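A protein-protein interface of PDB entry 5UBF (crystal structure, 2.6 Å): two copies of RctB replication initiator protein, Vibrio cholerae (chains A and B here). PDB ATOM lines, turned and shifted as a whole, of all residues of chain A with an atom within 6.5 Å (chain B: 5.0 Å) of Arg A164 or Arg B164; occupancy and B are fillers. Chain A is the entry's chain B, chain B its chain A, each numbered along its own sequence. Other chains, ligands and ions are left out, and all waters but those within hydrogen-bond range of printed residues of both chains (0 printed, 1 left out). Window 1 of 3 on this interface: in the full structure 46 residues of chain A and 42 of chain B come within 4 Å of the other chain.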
ATOM      1  N   ARG A  62     -14.182 -17.415   2.783  1.00  0.00           N
ATOM      2  CA  ARG A  62     -14.588 -17.062   1.429  1.00  0.00           C
ATOM      3  C   ARG A  62     -14.326 -18.222   0.483  1.00  0.00           C
ATOM      4  O   ARG A  62     -13.485 -19.088   0.738  1.00  0.00           O
ATOM      5  CB  ARG A  62     -13.878 -15.792   0.935  1.00  0.00           C
ATOM      6  CG  ARG A  62     -12.386 -15.790   1.155  1.00  0.00           C
ATOM      7  CD  ARG A  62     -11.701 -14.710   0.334  1.00  0.00           C
ATOM      8  NE  ARG A  62     -11.821 -13.372   0.907  1.00  0.00           N
ATOM      9  CZ  ARG A  62     -12.630 -12.423   0.445  1.00  0.00           C
ATOM     10  NH1 ARG A  62     -13.411 -12.658  -0.601  1.00  0.00           N
ATOM     11  NH2 ARG A  62     -12.656 -11.234   1.030  1.00  0.00           N
ATOM     12  N   SER A  64     -14.764 -19.337  -4.026  1.00  0.00           N
ATOM     13  CA  SER A  64     -15.227 -19.049  -5.377  1.00  0.00           C
ATOM     14  C   SER A  64     -16.580 -19.690  -5.651  1.00  0.00           C
ATOM     15  O   SER A  64     -17.288 -19.254  -6.564  1.00  0.00           O
ATOM     16  CB  SER A  64     -14.197 -19.521  -6.406  1.00  0.00           C
ATOM     17  OG  SER A  64     -13.869 -20.886  -6.213  1.00  0.00           O
ATOM     18  N   ILE A 135     -15.849 -28.041   1.150  1.00  0.00           N
ATOM     19  CA  ILE A 135     -14.637 -28.063   1.967  1.00  0.00           C
ATOM     20  C   ILE A 135     -13.417 -27.708   1.126  1.00  0.00           C
ATOM     21  O   ILE A 135     -12.511 -26.997   1.581  1.00  0.00           O
ATOM     22  CB  ILE A 135     -14.475 -29.441   2.637  1.00  0.00           C
ATOM     23  CG1 ILE A 135     -15.634 -29.711   3.598  1.00  0.00           C
ATOM     24  CG2 ILE A 135     -13.137 -29.540   3.358  1.00  0.00           C
ATOM     25  CD1 ILE A 135     -15.608 -31.098   4.199  1.00  0.00           C
ATOM     26  N   GLU A 136     -13.387 -28.177  -0.123  1.00  0.00           N
ATOM     27  CA  GLU A 136     -12.191 -28.055  -0.948  1.00  0.00           C
ATOM     28  C   GLU A 136     -11.928 -26.609  -1.359  1.00  0.00           C
ATOM     29  O   GLU A 136     -10.771 -26.178  -1.420  1.00  0.00           O
ATOM     30  CB  GLU A 136     -12.331 -28.946  -2.180  1.00  0.00           C
ATOM     31  CG  GLU A 136     -11.218 -28.808  -3.197  1.00  0.00           C
ATOM     32  CD  GLU A 136     -11.402 -29.746  -4.371  1.00  0.00           C
ATOM     33  OE1 GLU A 136     -12.381 -30.522  -4.361  1.00  0.00           O
ATOM     34  OE2 GLU A 136     -10.572 -29.708  -5.303  1.00  0.00           O
ATOM     35  N   PHE A 137     -12.982 -25.845  -1.643  1.00  0.00           N
ATOM     36  CA  PHE A 137     -12.837 -24.499  -2.180  1.00  0.00           C
ATOM     37  C   PHE A 137     -13.033 -23.412  -1.127  1.00  0.00           C
ATOM     38  O   PHE A 137     -13.272 -22.255  -1.482  1.00  0.00           O
ATOM     39  CB  PHE A 137     -13.808 -24.291  -3.342  1.00  0.00           C
ATOM     40  CG  PHE A 137     -13.338 -24.889  -4.637  1.00  0.00           C
ATOM     41  CD1 PHE A 137     -12.524 -24.164  -5.493  1.00  0.00           C
ATOM     42  CD2 PHE A 137     -13.708 -26.173  -4.998  1.00  0.00           C
ATOM     43  CE1 PHE A 137     -12.088 -24.709  -6.684  1.00  0.00           C
ATOM     44  CE2 PHE A 137     -13.275 -26.723  -6.189  1.00  0.00           C
ATOM     45  CZ  PHE A 137     -12.463 -25.991  -7.033  1.00  0.00           C
ATOM     46  N   THR A 138     -12.922 -23.750   0.153  1.00  0.00           N
ATOM     47  CA  THR A 138     -13.133 -22.791   1.228  1.00  0.00           C
ATOM     48  C   THR A 138     -11.795 -22.320   1.781  1.00  0.00           C
ATOM     49  O   THR A 138     -10.952 -23.135   2.173  1.00  0.00           O
ATOM     50  CB  THR A 138     -13.983 -23.397   2.347  1.00  0.00           C
ATOM     51  OG1 THR A 138     -15.312 -23.631   1.864  1.00  0.00           O
ATOM     52  CG2 THR A 138     -14.044 -22.455   3.536  1.00  0.00           C
ATOM     53  N   ASP A 139     -11.605 -21.005   1.806  1.00  0.00           N
ATOM     54  CA  ASP A 139     -10.425 -20.377   2.380  1.00  0.00           C
ATOM     55  C   ASP A 139     -10.813 -19.662   3.668  1.00  0.00           C
ATOM     56  O   ASP A 139     -11.756 -18.858   3.678  1.00  0.00           O
ATOM     57  CB  ASP A 139      -9.791 -19.388   1.399  1.00  0.00           C
ATOM     58  CG  ASP A 139      -8.919 -20.070   0.363  1.00  0.00           C
ATOM     59  OD1 ASP A 139      -8.129 -20.960   0.740  1.00  0.00           O
ATOM     60  OD2 ASP A 139      -9.025 -19.715  -0.830  1.00  0.00           O
ATOM     61  N   PHE A 140     -10.094 -19.967   4.745  1.00  0.00           N
ATOM     62  CA  PHE A 140     -10.239 -19.271   6.014  1.00  0.00           C
ATOM     63  C   PHE A 140      -9.076 -18.301   6.186  1.00  0.00           C
ATOM     64  O   PHE A 140      -7.981 -18.531   5.675  1.00  0.00           O
ATOM     65  CB  PHE A 140     -10.272 -20.252   7.187  1.00  0.00           C
ATOM     66  CG  PHE A 140     -11.385 -21.260   7.112  1.00  0.00           C
ATOM     67  CD1 PHE A 140     -12.645 -20.959   7.603  1.00  0.00           C
ATOM     68  CD2 PHE A 140     -11.168 -22.514   6.562  1.00  0.00           C
ATOM     69  CE1 PHE A 140     -13.670 -21.886   7.540  1.00  0.00           C
ATOM     70  CE2 PHE A 140     -12.189 -23.446   6.497  1.00  0.00           C
ATOM     71  CZ  PHE A 140     -13.442 -23.131   6.987  1.00  0.00           C
ATOM     72  N   ARG A 162      -3.782 -17.213   6.362  1.00  0.00           N
ATOM     73  CA  ARG A 162      -4.673 -17.679   5.305  1.00  0.00           C
ATOM     74  C   ARG A 162      -4.476 -19.184   5.164  1.00  0.00           C
ATOM     75  O   ARG A 162      -3.401 -19.642   4.764  1.00  0.00           O
ATOM     76  CB  ARG A 162      -4.398 -16.944   3.995  1.00  0.00           C
ATOM     77  CG  ARG A 162      -5.540 -16.996   2.983  1.00  0.00           C
ATOM     78  CD  ARG A 162      -5.488 -18.267   2.153  1.00  0.00           C
ATOM     79  NE  ARG A 162      -4.209 -18.401   1.463  1.00  0.00           N
ATOM     80  CZ  ARG A 162      -3.747 -19.542   0.963  1.00  0.00           C
ATOM     81  NH1 ARG A 162      -4.459 -20.653   1.084  1.00  0.00           N
ATOM     82  NH2 ARG A 162      -2.574 -19.572   0.348  1.00  0.00           N
ATOM     83  N   PHE A 163      -5.516 -19.945   5.489  1.00  0.00           N
ATOM     84  CA  PHE A 163      -5.444 -21.392   5.596  1.00  0.00           C
ATOM     85  C   PHE A 163      -6.504 -22.047   4.721  1.00  0.00           C
ATOM     86  O   PHE A 163      -7.587 -21.493   4.492  1.00  0.00           O
ATOM     87  CB  PHE A 163      -5.613 -21.842   7.059  1.00  0.00           C
ATOM     88  CG  PHE A 163      -5.781 -23.327   7.224  1.00  0.00           C
ATOM     89  CD1 PHE A 163      -4.698 -24.181   7.093  1.00  0.00           C
ATOM     90  CD2 PHE A 163      -7.022 -23.866   7.519  1.00  0.00           C
ATOM     91  CE1 PHE A 163      -4.851 -25.546   7.248  1.00  0.00           C
ATOM     92  CE2 PHE A 163      -7.182 -25.230   7.677  1.00  0.00           C
ATOM     93  CZ  PHE A 163      -6.094 -26.071   7.540  1.00  0.00           C
ATOM     94  N   ARG A 164      -6.170 -23.247   4.251  1.00  0.00           N
ATOM     95  CA  ARG A 164      -7.020 -24.051   3.387  1.00  0.00           C
ATOM     96  C   ARG A 164      -6.733 -25.510   3.708  1.00  0.00           C
ATOM     97  O   ARG A 164      -5.567 -25.900   3.804  1.00  0.00           O
ATOM     98  CB  ARG A 164      -6.734 -23.740   1.915  1.00  0.00           C
ATOM     99  CG  ARG A 164      -7.673 -24.364   0.903  1.00  0.00           C
ATOM    100  CD  ARG A 164      -7.209 -23.976  -0.491  1.00  0.00           C
ATOM    101  NE  ARG A 164      -8.073 -24.471  -1.557  1.00  0.00           N
ATOM    102  CZ  ARG A 164      -9.004 -23.742  -2.163  1.00  0.00           C
ATOM    103  NH1 ARG A 164      -9.199 -22.480  -1.804  1.00  0.00           N
ATOM    104  NH2 ARG A 164      -9.737 -24.273  -3.131  1.00  0.00           N
ATOM    105  N   PHE A 165      -7.788 -26.304   3.891  1.00  0.00           N
ATOM    106  CA  PHE A 165      -7.608 -27.691   4.313  1.00  0.00           C
ATOM    107  C   PHE A 165      -6.880 -28.506   3.251  1.00  0.00           C
ATOM    108  O   PHE A 165      -5.806 -29.063   3.503  1.00  0.00           O
ATOM    109  CB  PHE A 165      -8.962 -28.321   4.640  1.00  0.00           C
ATOM    110  CG  PHE A 165      -9.420 -28.082   6.050  1.00  0.00           C
ATOM    111  CD1 PHE A 165      -8.829 -28.755   7.106  1.00  0.00           C
ATOM    112  CD2 PHE A 165     -10.448 -27.195   6.319  1.00  0.00           C
ATOM    113  CE1 PHE A 165      -9.248 -28.542   8.405  1.00  0.00           C
ATOM    114  CE2 PHE A 165     -10.874 -26.978   7.615  1.00  0.00           C
ATOM    115  CZ  PHE A 165     -10.272 -27.654   8.659  1.00  0.00           C
ATOM    116  N   LEU A 166      -7.454 -28.590   2.055  1.00  0.00           N
ATOM    117  CA  LEU A 166      -6.930 -29.434   0.986  1.00  0.00           C
ATOM    118  C   LEU A 166      -6.052 -28.592   0.068  1.00  0.00           C
ATOM    119  O   LEU A 166      -6.554 -27.750  -0.683  1.00  0.00           O
ATOM    120  CB  LEU A 166      -8.072 -30.088   0.211  1.00  0.00           C
ATOM    121  CG  LEU A 166      -8.950 -31.037   1.030  1.00  0.00           C
ATOM    122  CD1 LEU A 166     -10.135 -31.520   0.210  1.00  0.00           C
ATOM    123  CD2 LEU A 166      -8.127 -32.213   1.535  1.00  0.00           C
ATOM    124  N   ALA A 167      -4.740 -28.821   0.132  1.00  0.00           N
ATOM    125  CA  ALA A 167      -3.829 -28.129  -0.772  1.00  0.00           C
ATOM    126  C   ALA A 167      -4.002 -28.603  -2.206  1.00  0.00           C
ATOM    127  O   ALA A 167      -3.818 -27.820  -3.145  1.00  0.00           O
ATOM    128  CB  ALA A 167      -2.383 -28.326  -0.321  1.00  0.00           C
ATOM    129  N   ARG A 168      -4.353 -29.874  -2.399  1.00  0.00           N
ATOM    130  CA  ARG A 168      -4.546 -30.410  -3.737  1.00  0.00           C
ATOM    131  C   ARG A 168      -5.565 -31.537  -3.674  1.00  0.00           C
ATOM    132  O   ARG A 168      -5.719 -32.195  -2.643  1.00  0.00           O
ATOM    133  CB  ARG A 168      -3.226 -30.912  -4.334  1.00  0.00           C
ATOM    134  CG  ARG A 168      -3.237 -31.092  -5.842  1.00  0.00           C
ATOM    135  CD  ARG A 168      -2.003 -31.845  -6.306  1.00  0.00           C
ATOM    136  NE  ARG A 168      -1.818 -31.762  -7.750  1.00  0.00           N
ATOM    137  CZ  ARG A 168      -0.976 -32.524  -8.439  1.00  0.00           C
ATOM    138  NH1 ARG A 168      -0.244 -33.438  -7.817  1.00  0.00           N
ATOM    139  NH2 ARG A 168      -0.869 -32.378  -9.753  1.00  0.00           N
ATOM    140  N   TRP A 196      -3.445 -32.727   1.846  1.00  0.00           N
ATOM    141  CA  TRP A 196      -3.787 -31.775   2.888  1.00  0.00           C
ATOM    142  C   TRP A 196      -2.751 -30.658   2.958  1.00  0.00           C
ATOM    143  O   TRP A 196      -1.664 -30.737   2.378  1.00  0.00           O
ATOM    144  CB  TRP A 196      -3.872 -32.470   4.247  1.00  0.00           C
ATOM    145  CG  TRP A 196      -4.916 -33.534   4.340  1.00  0.00           C
ATOM    146  CD1 TRP A 196      -4.779 -34.849   4.004  1.00  0.00           C
ATOM    147  CD2 TRP A 196      -6.258 -33.379   4.817  1.00  0.00           C
ATOM    148  NE1 TRP A 196      -5.955 -35.521   4.236  1.00  0.00           N
ATOM    149  CE2 TRP A 196      -6.878 -34.641   4.736  1.00  0.00           C
ATOM    150  CE3 TRP A 196      -6.995 -32.295   5.302  1.00  0.00           C
ATOM    151  CZ2 TRP A 196      -8.200 -34.848   5.120  1.00  0.00           C
ATOM    152  CZ3 TRP A 196      -8.308 -32.503   5.683  1.00  0.00           C
ATOM    153  CH2 TRP A 196      -8.896 -33.769   5.590  1.00  0.00           C
ATOM    154  N   GLU A 197      -3.106 -29.603   3.681  1.00  0.00           N
ATOM    155  CA  GLU A 197      -2.136 -28.572   4.013  1.00  0.00           C
ATOM    156  C   GLU A 197      -0.980 -29.218   4.772  1.00  0.00           C
ATOM    157  O   GLU A 197      -1.221 -30.011   5.692  1.00  0.00           O
ATOM    158  CB  GLU A 197      -2.794 -27.474   4.851  1.00  0.00           C
ATOM    159  CG  GLU A 197      -1.980 -26.193   4.982  1.00  0.00           C
ATOM    160  CD  GLU A 197      -0.889 -26.293   6.031  1.00  0.00           C
ATOM    161  OE1 GLU A 197      -1.076 -27.041   7.014  1.00  0.00           O
ATOM    162  OE2 GLU A 197       0.157 -25.630   5.870  1.00  0.00           O
ATOM    163  N   PHE A 200      -0.770 -28.906   8.818  1.00  0.00           N
ATOM    164  CA  PHE A 200      -1.950 -29.587   9.340  1.00  0.00           C
ATOM    165  C   PHE A 200      -1.854 -31.092   9.133  1.00  0.00           C
ATOM    166  O   PHE A 200      -2.237 -31.873  10.012  1.00  0.00           O
ATOM    167  CB  PHE A 200      -3.214 -29.035   8.681  1.00  0.00           C
ATOM    168  CG  PHE A 200      -4.484 -29.660   9.188  1.00  0.00           C
ATOM    169  CD1 PHE A 200      -5.106 -29.169  10.323  1.00  0.00           C
ATOM    170  CD2 PHE A 200      -5.055 -30.738   8.531  1.00  0.00           C
ATOM    171  CE1 PHE A 200      -6.271 -29.741  10.795  1.00  0.00           C
ATOM    172  CE2 PHE A 200      -6.221 -31.315   8.999  1.00  0.00           C
ATOM    173  CZ  PHE A 200      -6.829 -30.815  10.133  1.00  0.00           C
ATOM    174  N   GLU B 136      -2.301 -15.853  -4.725  1.00  0.00           N
ATOM    175  CA  GLU B 136      -2.568 -16.641  -3.526  1.00  0.00           C
ATOM    176  C   GLU B 136      -3.956 -17.272  -3.557  1.00  0.00           C
ATOM    177  O   GLU B 136      -4.138 -18.406  -3.097  1.00  0.00           O
ATOM    178  CB  GLU B 136      -2.403 -15.760  -2.287  1.00  0.00           C
ATOM    179  CG  GLU B 136      -2.746 -16.431  -0.970  1.00  0.00           C
ATOM    180  CD  GLU B 136      -2.543 -15.505   0.213  1.00  0.00           C
ATOM    181  OE1 GLU B 136      -2.004 -14.396   0.012  1.00  0.00           O
ATOM    182  OE2 GLU B 136      -2.923 -15.882   1.341  1.00  0.00           O
ATOM    183  N   PHE B 137      -4.949 -16.563  -4.094  1.00  0.00           N
ATOM    184  CA  PHE B 137      -6.331 -17.019  -4.075  1.00  0.00           C
ATOM    185  C   PHE B 137      -6.769 -17.655  -5.391  1.00  0.00           C
ATOM    186  O   PHE B 137      -7.973 -17.792  -5.632  1.00  0.00           O
ATOM    187  CB  PHE B 137      -7.265 -15.859  -3.719  1.00  0.00           C
ATOM    188  CG  PHE B 137      -7.215 -15.462  -2.273  1.00  0.00           C
ATOM    189  CD1 PHE B 137      -8.019 -16.097  -1.341  1.00  0.00           C
ATOM    190  CD2 PHE B 137      -6.369 -14.453  -1.845  1.00  0.00           C
ATOM    191  CE1 PHE B 137      -7.978 -15.735  -0.008  1.00  0.00           C
ATOM    192  CE2 PHE B 137      -6.321 -14.087  -0.513  1.00  0.00           C
ATOM    193  CZ  PHE B 137      -7.126 -14.730   0.408  1.00  0.00           C
ATOM    194  N   THR B 138      -5.828 -18.055  -6.242  1.00  0.00           N
ATOM    195  CA  THR B 138      -6.153 -18.630  -7.540  1.00  0.00           C
ATOM    196  C   THR B 138      -6.070 -20.150  -7.473  1.00  0.00           C
ATOM    197  O   THR B 138      -5.034 -20.706  -7.097  1.00  0.00           O
ATOM    198  CB  THR B 138      -5.222 -18.098  -8.630  1.00  0.00           C
ATOM    199  OG1 THR B 138      -5.437 -16.692  -8.801  1.00  0.00           O
ATOM    200  CG2 THR B 138      -5.500 -18.804  -9.941  1.00  0.00           C
ATOM    201  N   ASP B 139      -7.162 -20.812  -7.837  1.00  0.00           N
ATOM    202  CA  ASP B 139      -7.209 -22.257  -7.996  1.00  0.00           C
ATOM    203  C   ASP B 139      -7.278 -22.603  -9.476  1.00  0.00           C
ATOM    204  O   ASP B 139      -8.032 -21.984 -10.234  1.00  0.00           O
ATOM    205  CB  ASP B 139      -8.417 -22.857  -7.270  1.00  0.00           C
ATOM    206  CG  ASP B 139      -8.231 -22.906  -5.771  1.00  0.00           C
ATOM    207  OD1 ASP B 139      -7.158 -23.359  -5.322  1.00  0.00           O
ATOM    208  OD2 ASP B 139      -9.155 -22.489  -5.043  1.00  0.00           O
ATOM    209  N   ARG B 162      -7.153 -30.478  -9.169  1.00  0.00           N
ATOM    210  CA  ARG B 162      -7.362 -29.136  -8.636  1.00  0.00           C
ATOM    211  C   ARG B 162      -6.100 -28.722  -7.886  1.00  0.00           C
ATOM    212  O   ARG B 162      -5.791 -29.268  -6.822  1.00  0.00           O
ATOM    213  CB  ARG B 162      -8.596 -29.097  -7.735  1.00  0.00           C
ATOM    214  CG  ARG B 162      -9.167 -27.704  -7.491  1.00  0.00           C
ATOM    215  CD  ARG B 162      -8.524 -27.050  -6.284  1.00  0.00           C
ATOM    216  NE  ARG B 162      -8.580 -27.925  -5.119  1.00  0.00           N
ATOM    217  CZ  ARG B 162      -7.767 -27.825  -4.072  1.00  0.00           C
ATOM    218  NH1 ARG B 162      -6.830 -26.887  -4.048  1.00  0.00           N
ATOM    219  NH2 ARG B 162      -7.886 -28.665  -3.055  1.00  0.00           N
ATOM    220  N   PHE B 163      -5.381 -27.752  -8.441  1.00  0.00           N
ATOM    221  CA  PHE B 163      -4.064 -27.357  -7.975  1.00  0.00           C
ATOM    222  C   PHE B 163      -4.082 -25.912  -7.494  1.00  0.00           C
ATOM    223  O   PHE B 163      -4.888 -25.092  -7.946  1.00  0.00           O
ATOM    224  CB  PHE B 163      -3.023 -27.529  -9.094  1.00  0.00           C
ATOM    225  CG  PHE B 163      -1.642 -27.080  -8.718  1.00  0.00           C
ATOM    226  CD1 PHE B 163      -0.816 -27.894  -7.958  1.00  0.00           C
ATOM    227  CD2 PHE B 163      -1.163 -25.847  -9.133  1.00  0.00           C
ATOM    228  CE1 PHE B 163       0.459 -27.484  -7.615  1.00  0.00           C
ATOM    229  CE2 PHE B 163       0.110 -25.431  -8.792  1.00  0.00           C
ATOM    230  CZ  PHE B 163       0.922 -26.251  -8.032  1.00  0.00           C
ATOM    231  N   ARG B 164      -3.168 -25.612  -6.575  1.00  0.00           N
ATOM    232  CA  ARG B 164      -3.029 -24.285  -5.994  1.00  0.00           C
ATOM    233  C   ARG B 164      -1.568 -24.092  -5.619  1.00  0.00           C
ATOM    234  O   ARG B 164      -0.964 -24.983  -5.017  1.00  0.00           O
ATOM    235  CB  ARG B 164      -3.933 -24.138  -4.768  1.00  0.00           C
ATOM    236  CG  ARG B 164      -3.950 -22.769  -4.131  1.00  0.00           C
ATOM    237  CD  ARG B 164      -4.777 -22.825  -2.863  1.00  0.00           C
ATOM    238  NE  ARG B 164      -5.006 -21.511  -2.273  1.00  0.00           N
ATOM    239  CZ  ARG B 164      -6.053 -20.744  -2.555  1.00  0.00           C
ATOM    240  NH1 ARG B 164      -6.965 -21.156  -3.423  1.00  0.00           N
ATOM    241  NH2 ARG B 164      -6.186 -19.562  -1.968  1.00  0.00           N
ATOM    242  N   PHE B 165      -1.001 -22.939  -5.985  1.00  0.00           N
ATOM    243  CA  PHE B 165       0.422 -22.709  -5.743  1.00  0.00           C
ATOM    244  C   PHE B 165       0.729 -22.632  -4.253  1.00  0.00           C
ATOM    245  O   PHE B 165       1.642 -23.306  -3.762  1.00  0.00           O
ATOM    246  CB  PHE B 165       0.879 -21.432  -6.449  1.00  0.00           C
ATOM    247  CG  PHE B 165       1.258 -21.637  -7.885  1.00  0.00           C
ATOM    248  CD1 PHE B 165       2.291 -22.495  -8.224  1.00  0.00           C
ATOM    249  CD2 PHE B 165       0.593 -20.964  -8.897  1.00  0.00           C
ATOM    250  CE1 PHE B 165       2.646 -22.689  -9.546  1.00  0.00           C
ATOM    251  CE2 PHE B 165       0.944 -21.151 -10.220  1.00  0.00           C
ATOM    252  CZ  PHE B 165       1.973 -22.015 -10.543  1.00  0.00           C
ATOM    253  N   LEU B 166      -0.018 -21.815  -3.516  1.00  0.00           N
ATOM    254  CA  LEU B 166       0.238 -21.580  -2.100  1.00  0.00           C
ATOM    255  C   LEU B 166      -0.785 -22.350  -1.272  1.00  0.00           C
ATOM    256  O   LEU B 166      -1.972 -22.013  -1.268  1.00  0.00           O
ATOM    257  CB  LEU B 166       0.195 -20.087  -1.784  1.00  0.00           C
ATOM    258  CG  LEU B 166       1.250 -19.244  -2.503  1.00  0.00           C
ATOM    259  CD1 LEU B 166       1.089 -17.768  -2.175  1.00  0.00           C
ATOM    260  CD2 LEU B 166       2.647 -19.724  -2.146  1.00  0.00           C
ATOM    261  N   ALA B 167      -0.318 -23.387  -0.573  1.00  0.00           N
ATOM    262  CA  ALA B 167      -1.197 -24.125   0.326  1.00  0.00           C
ATOM    263  C   ALA B 167      -1.580 -23.282   1.534  1.00  0.00           C
ATOM    264  O   ALA B 167      -2.720 -23.350   2.010  1.00  0.00           O
ATOM    265  CB  ALA B 167      -0.523 -25.422   0.773  1.00  0.00           C
ATOM    266  N   GLU B 197       2.497 -25.700  -2.304  1.00  0.00           N
ATOM    267  CA  GLU B 197       1.872 -27.003  -2.479  1.00  0.00           C
ATOM    268  C   GLU B 197       2.938 -28.086  -2.350  1.00  0.00           C
ATOM    269  O   GLU B 197       4.026 -27.944  -2.919  1.00  0.00           O
ATOM    270  CB  GLU B 197       1.178 -27.081  -3.839  1.00  0.00           C
ATOM    271  CG  GLU B 197       0.258 -28.280  -4.020  1.00  0.00           C
ATOM    272  CD  GLU B 197       0.985 -29.499  -4.554  1.00  0.00           C
ATOM    273  OE1 GLU B 197       2.036 -29.326  -5.205  1.00  0.00           O
ATOM    274  OE2 GLU B 197       0.505 -30.630  -4.322  1.00  0.00           O
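Phe A137 touches Asp B139, and with the chains exchanged Asp A139 touches Phe B137.
Asp A139 touches Arg B164, and with the chains exchanged Arg A164 touches Asp B139.
Arg A162 touches Ala B167, and with the chains exchanged Ala A167 touches Arg B162.
Arg A164 touches its own counterpart, Arg B164.
11 positions are printed for both chains.
Of the 19 pairs that touch across the chains among the printed residues, 16 have their exchanged pair printed and touching as well.
Among the printed residues, merely in contact across the chains: Arg A168 with Arg B162 (3.3 Å), Arg A168 with Glu B197 (3.4 Å), Arg A162 with Arg B164 (3.5 Å), Ala A167 with Ala B167 (3.6 Å), Arg A164 with Arg B162 (3.7 Å), Phe A137 with Arg B162 (3.7 Å), Arg A162 with Phe B137 (3.8 Å), Phe A137 with Asp B139 (3.8 Å), Asp A139 with Phe B137 (3.8 Å) and Arg A62 with Phe B137 (3.9 Å).
The side-chain carboxylate of Asp B139 lies within salt-bridge range of the guanidinium group of Arg B164.
The backbone carbonyl oxygen of Leu B166 is in hydrogen-bond range of the guanidinium group of Arg B164 (3.2 Å).
The backbone NH (N) of Glu B197 sits at hydrogen-bond distance from the backbone carbonyl oxygen (O) of Phe B165.
NH2 of Arg A164 lies within hydrogen-bond range of O of Glu A136 (2.8 Å).
OD1 of Asp A139 lies within salt-bridge range of NH1 of Arg A162, at 3.7 Å.
The guanidinium group (NH1) of Arg A164 is in salt-bridge range of the side-chain carboxylate (OD2) of Asp A139.
Of the printed residues of chain B, Asp A139 touches Phe B137 and Arg B164.
Of the printed residues of chain B, Arg A162 touches Glu B136 (2.8 Å), Phe B137 (3.8 Å), Arg B164 (3.5 Å), Leu B166 (3.0 Å) and Ala B167 (3.3 Å).
Phe A163 touches none of the printed residues of chain B.
Arg A164 touches three residues of chain B.
Glu A197 touches none of the printed residues of chain B.
The nearest printed residue of chain B that does not touch Ala A167 is Arg B164 (4.03 Å).
The guanidinium group (NE) of Arg A162 lies within salt-bridge range of the side-chain carboxylate (OE2) of Glu B136 (2.8 Å).
OD2 of Asp B139 lies within salt-bridge range of NH2 of Arg A164, 2.7 Å away.
OE2 of Glu A136 lies within salt-bridge range of NE of Arg B162 (2.7 Å).
The backbone carbonyl oxygen of Leu A166 is in hydrogen-bond range of the guanidinium group of Arg B162, 2.9 Å away.
The guanidinium group (NH1) of Arg B162 is in hydrogen-bond range of the backbone carbonyl oxygen (O) of Ala A167 (3.3 Å).
The guanidinium group of Arg B164 is in salt-bridge range of the side-chain carboxylate of Asp A139, 3.1 Å away.
The backbone carbonyl oxygen of Leu B166 lies within hydrogen-bond range of the guanidinium group of Arg A162, 3.0 Å away.
The guanidinium group of Arg A162 sits at hydrogen-bond distance from the backbone carbonyl oxygen of Ala B167.
The guanidinium group of Arg A164 lies close to the guanidinium group of Arg B164 (3.1 Å).
Printed residues of chain A that touch a printed residue of chain B: Arg A62, Glu A136, Phe A137, Asp A139, Arg A162, Arg A164, Leu A166, Ala A167 and Arg A168.
Of the 11 printed residues of chain B, 8 touch a printed residue of chain A.
Printed residues of chain B that touch a printed residue of chain A: Glu B136, Phe B137, Asp B139, Arg B162, Arg B164, Leu B166, Ala B167 and Glu B197.
Among the printed residues, Asp or Glu carboxylates within 4 Å of a Lys or Arg side-chain nitrogen of the other chain: Glu A136 with Arg B162 (2.7 Å), Asp A139 with Arg B164 (3.1 Å), Arg A162 with Glu B136 (2.8 Å) and Arg A164 with Asp B139 (2.7 Å).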
